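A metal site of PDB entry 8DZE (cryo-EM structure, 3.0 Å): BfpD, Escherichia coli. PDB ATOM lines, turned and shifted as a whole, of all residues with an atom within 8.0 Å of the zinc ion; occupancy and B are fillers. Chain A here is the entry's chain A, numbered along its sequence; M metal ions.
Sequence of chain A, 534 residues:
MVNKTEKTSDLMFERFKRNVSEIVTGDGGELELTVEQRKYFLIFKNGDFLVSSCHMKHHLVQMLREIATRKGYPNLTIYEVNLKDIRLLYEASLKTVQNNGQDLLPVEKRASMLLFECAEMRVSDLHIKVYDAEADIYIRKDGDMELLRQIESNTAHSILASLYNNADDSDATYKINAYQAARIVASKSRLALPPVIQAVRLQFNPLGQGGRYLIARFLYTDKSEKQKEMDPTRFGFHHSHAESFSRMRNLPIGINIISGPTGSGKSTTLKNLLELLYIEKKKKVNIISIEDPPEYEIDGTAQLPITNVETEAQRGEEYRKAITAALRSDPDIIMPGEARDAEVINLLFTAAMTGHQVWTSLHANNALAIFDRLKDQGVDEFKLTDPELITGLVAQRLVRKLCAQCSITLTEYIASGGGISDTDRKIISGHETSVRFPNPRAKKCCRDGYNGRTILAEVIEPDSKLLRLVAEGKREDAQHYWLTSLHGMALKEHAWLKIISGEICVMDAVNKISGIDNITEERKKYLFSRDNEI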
ATOM      1  N   LEU A 402     -30.844   5.865  26.962  1.00  0.00           N
ATOM      2  CA  LEU A 402     -30.150   4.578  26.954  1.00  0.00           C
ATOM      3  C   LEU A 402     -31.145   3.437  26.708  1.00  0.00           C
ATOM      4  O   LEU A 402     -32.298   3.489  27.122  1.00  0.00           O
ATOM      5  CB  LEU A 402     -29.425   4.357  28.273  1.00  0.00           C
ATOM      6  CG  LEU A 402     -28.532   5.491  28.773  1.00  0.00           C
ATOM      7  CD1 LEU A 402     -27.824   5.093  30.055  1.00  0.00           C
ATOM      8  CD2 LEU A 402     -27.544   5.901  27.704  1.00  0.00           C
ATOM      9  N   CYS A 403     -30.668   2.410  26.016  1.00  0.00           N
ATOM     10  CA  CYS A 403     -31.477   1.218  25.788  1.00  0.00           C
ATOM     11  C   CYS A 403     -31.640   0.439  27.089  1.00  0.00           C
ATOM     12  O   CYS A 403     -30.673   0.243  27.830  1.00  0.00           O
ATOM     13  CB  CYS A 403     -30.857   0.342  24.712  1.00  0.00           C
ATOM     14  SG  CYS A 403     -31.731  -1.206  24.401  1.00  0.00           S
ATOM     15  N   ALA A 404     -32.867   0.001  27.359  1.00  0.00           N
ATOM     16  CA  ALA A 404     -33.130  -0.708  28.611  1.00  0.00           C
ATOM     17  C   ALA A 404     -32.587  -2.127  28.587  1.00  0.00           C
ATOM     18  O   ALA A 404     -32.267  -2.680  29.640  1.00  0.00           O
ATOM     19  CB  ALA A 404     -34.639  -0.718  28.891  1.00  0.00           C
ATOM     20  N   GLN A 405     -32.478  -2.726  27.401  1.00  0.00           N
ATOM     21  CA  GLN A 405     -32.012  -4.109  27.312  1.00  0.00           C
ATOM     22  C   GLN A 405     -30.520  -4.222  27.601  1.00  0.00           C
ATOM     23  O   GLN A 405     -30.082  -5.166  28.278  1.00  0.00           O
ATOM     24  CB  GLN A 405     -32.327  -4.685  25.935  1.00  0.00           C
ATOM     25  CG  GLN A 405     -33.690  -5.361  25.847  1.00  0.00           C
ATOM     26  CD  GLN A 405     -34.821  -4.379  25.665  1.00  0.00           C
ATOM     27  OE1 GLN A 405     -35.049  -3.869  24.563  1.00  0.00           O
ATOM     28  NE2 GLN A 405     -35.549  -4.101  26.743  1.00  0.00           N
ATOM     29  N   CYS A 406     -29.722  -3.272  27.114  1.00  0.00           N
ATOM     30  CA  CYS A 406     -28.269  -3.299  27.295  1.00  0.00           C
ATOM     31  C   CYS A 406     -27.864  -2.080  28.111  1.00  0.00           C
ATOM     32  O   CYS A 406     -27.595  -1.003  27.572  1.00  0.00           O
ATOM     33  CB  CYS A 406     -27.547  -3.339  25.940  1.00  0.00           C
ATOM     34  SG  CYS A 406     -28.129  -2.158  24.704  1.00  0.00           S
ATOM     35  N   SER A 407     -27.812  -2.246  29.430  1.00  0.00           N
ATOM     36  CA  SER A 407     -27.349  -1.217  30.337  1.00  0.00           C
ATOM     37  C   SER A 407     -26.369  -1.826  31.339  1.00  0.00           C
ATOM     38  O   SER A 407     -26.498  -2.982  31.732  1.00  0.00           O
ATOM     39  CB  SER A 407     -28.517  -0.552  31.088  1.00  0.00           C
ATOM     40  OG  SER A 407     -29.359   0.158  30.190  1.00  0.00           O
ATOM     41  N   ASN A 439     -23.974   0.513  26.795  1.00  0.00           N
ATOM     42  CA  ASN A 439     -23.316  -0.771  26.678  1.00  0.00           C
ATOM     43  C   ASN A 439     -22.699  -0.919  25.298  1.00  0.00           C
ATOM     44  O   ASN A 439     -23.424  -0.827  24.293  1.00  0.00           O
ATOM     45  CB  ASN A 439     -24.293  -1.900  26.948  1.00  0.00           C
ATOM     46  CG  ASN A 439     -23.607  -3.252  27.043  1.00  0.00           C
ATOM     47  OD1 ASN A 439     -22.583  -3.397  27.710  1.00  0.00           O
ATOM     48  ND2 ASN A 439     -24.176  -4.253  26.375  1.00  0.00           N
ATOM     49  N   ALA A 442     -22.466  -3.593  20.474  1.00  0.00           N
ATOM     50  CA  ALA A 442     -23.531  -3.564  19.466  1.00  0.00           C
ATOM     51  C   ALA A 442     -24.323  -4.873  19.443  1.00  0.00           C
ATOM     52  O   ALA A 442     -24.271  -5.660  18.492  1.00  0.00           O
ATOM     53  CB  ALA A 442     -22.962  -3.237  18.079  1.00  0.00           C
ATOM     54  N   LYS A 443     -25.059  -5.100  20.535  1.00  0.00           N
ATOM     55  CA  LYS A 443     -25.844  -6.313  20.689  1.00  0.00           C
ATOM     56  C   LYS A 443     -27.028  -6.327  19.717  1.00  0.00           C
ATOM     57  O   LYS A 443     -27.198  -5.434  18.875  1.00  0.00           O
ATOM     58  CB  LYS A 443     -26.313  -6.462  22.132  1.00  0.00           C
ATOM     59  CG  LYS A 443     -25.371  -5.881  23.164  1.00  0.00           C
ATOM     60  CD  LYS A 443     -25.352  -6.714  24.432  1.00  0.00           C
ATOM     61  CE  LYS A 443     -26.764  -6.916  24.974  1.00  0.00           C
ATOM     62  NZ  LYS A 443     -26.817  -8.040  25.947  1.00  0.00           N
ATOM     63  N   LYS A 444     -27.860  -7.362  19.848  1.00  0.00           N
ATOM     64  CA  LYS A 444     -28.953  -7.593  18.892  1.00  0.00           C
ATOM     65  C   LYS A 444     -29.983  -6.468  18.931  1.00  0.00           C
ATOM     66  O   LYS A 444     -30.469  -6.037  17.883  1.00  0.00           O
ATOM     67  CB  LYS A 444     -29.613  -8.933  19.175  1.00  0.00           C
ATOM     68  N   CYS A 445     -30.319  -5.988  20.124  1.00  0.00           N
ATOM     69  CA  CYS A 445     -31.256  -4.872  20.231  1.00  0.00           C
ATOM     70  C   CYS A 445     -30.594  -3.588  19.767  1.00  0.00           C
ATOM     71  O   CYS A 445     -29.360  -3.473  19.711  1.00  0.00           O
ATOM     72  CB  CYS A 445     -31.732  -4.700  21.673  1.00  0.00           C
ATOM     73  SG  CYS A 445     -30.390  -4.450  22.849  1.00  0.00           S
ATOM     74  N   CYS A 446     -31.440  -2.615  19.395  1.00  0.00           N
ATOM     75  CA  CYS A 446     -31.080  -1.238  19.072  1.00  0.00           C
ATOM     76  C   CYS A 446     -29.908  -1.110  18.109  1.00  0.00           C
ATOM     77  O   CYS A 446     -29.649  -2.024  17.307  1.00  0.00           O
ATOM     78  CB  CYS A 446     -30.816  -0.431  20.354  1.00  0.00           C
ATOM     79  SG  CYS A 446     -29.399  -0.898  21.390  1.00  0.00           S
ATOM     80  N   ARG A 447     -29.202   0.019  18.147  1.00  0.00           N
ATOM     81  CA  ARG A 447     -28.077   0.251  17.250  1.00  0.00           C
ATOM     82  C   ARG A 447     -26.751   0.371  18.003  1.00  0.00           C
ATOM     83  O   ARG A 447     -25.811  -0.379  17.719  1.00  0.00           O
ATOM     84  CB  ARG A 447     -28.318   1.509  16.405  1.00  0.00           C
ATOM     85  N   ASP A 448     -26.653   1.290  18.971  1.00  0.00           N
ATOM     86  CA  ASP A 448     -25.411   1.504  19.698  1.00  0.00           C
ATOM     87  C   ASP A 448     -25.670   1.738  21.186  1.00  0.00           C
ATOM     88  O   ASP A 448     -24.935   2.502  21.835  1.00  0.00           O
ATOM     89  CB  ASP A 448     -24.625   2.678  19.114  1.00  0.00           C
ATOM     90  CG  ASP A 448     -25.523   3.816  18.667  1.00  0.00           C
ATOM     91  OD1 ASP A 448     -26.763   3.637  18.673  1.00  0.00           O
ATOM     92  OD2 ASP A 448     -24.999   4.896  18.316  1.00  0.00           O
ATOM     93  N   GLY A 449     -26.687   1.101  21.745  1.00  0.00           N
ATOM     94  CA  GLY A 449     -27.051   1.291  23.126  1.00  0.00           C
ATOM     95  C   GLY A 449     -27.959   2.458  23.403  1.00  0.00           C
ATOM     96  O   GLY A 449     -28.243   2.744  24.575  1.00  0.00           O
ATOM     97  N   TYR A 450     -28.434   3.154  22.364  1.00  0.00           N
ATOM     98  CA  TYR A 450     -29.346   4.279  22.513  1.00  0.00           C
ATOM     99  C   TYR A 450     -30.658   3.964  21.801  1.00  0.00           C
ATOM    100  O   TYR A 450     -30.652   3.394  20.702  1.00  0.00           O
ATOM    101  CB  TYR A 450     -28.742   5.559  21.948  1.00  0.00           C
ATOM    102  CG  TYR A 450     -27.534   6.054  22.709  1.00  0.00           C
ATOM    103  CD1 TYR A 450     -27.672   6.888  23.810  1.00  0.00           C
ATOM    104  CD2 TYR A 450     -26.245   5.702  22.318  1.00  0.00           C
ATOM    105  CE1 TYR A 450     -26.577   7.342  24.517  1.00  0.00           C
ATOM    106  CE2 TYR A 450     -25.141   6.155  23.014  1.00  0.00           C
ATOM    107  CZ  TYR A 450     -25.312   6.976  24.114  1.00  0.00           C
ATOM    108  OH  TYR A 450     -24.208   7.431  24.800  1.00  0.00           O
ATOM    109  N   ASN A 451     -31.770   4.326  22.434  1.00  0.00           N
ATOM    110  CA  ASN A 451     -33.108   4.038  21.919  1.00  0.00           C
ATOM    111  C   ASN A 451     -33.897   5.354  21.933  1.00  0.00           C
ATOM    112  O   ASN A 451     -34.539   5.678  22.935  1.00  0.00           O
ATOM    113  CB  ASN A 451     -33.783   2.949  22.757  1.00  0.00           C
ATOM    114  CG  ASN A 451     -35.184   2.600  22.255  1.00  0.00           C
ATOM    115  OD1 ASN A 451     -35.633   3.064  21.211  1.00  0.00           O
ATOM    116  ND2 ASN A 451     -35.884   1.764  23.020  1.00  0.00           N
HETATM  117 ZN    ZN M   1     -29.951  -2.187  23.257  1.00  0.00          ZN
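The backbone NH (N) of Cys 403 lies within hydrogen-bond range of the backbone carbonyl oxygen (O) of Gly 449 (2.8 Å).
O of Cys 403 is in hydrogen-bond range of OG of Ser 407 (2.7 Å).
The side-chain sulfur (SG) of Cys 446 sits close to the backbone NH (N) of Gly 449.
N of Gln 405 sits close to SG of Cys 403, at 3.4 Å.
Within 4 Å of the zinc ion: Cys 403, Cys 406, Cys 445 and Cys 446.
The nearest printed residue that does not touch the zinc ion is Gln 405 (4.4 Å).
SG of Cys 406 binds the zinc ion (2.3 Å).
SG of Cys 403 is bound to the zinc ion, at 2.3 Å.
The zinc ion is bound by the side-chain sulfur (SG) of Cys 446 (2.3 Å).
SG of Cys 445 is bound to the zinc ion.
The zinc ion has four donor atoms within binding distance.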
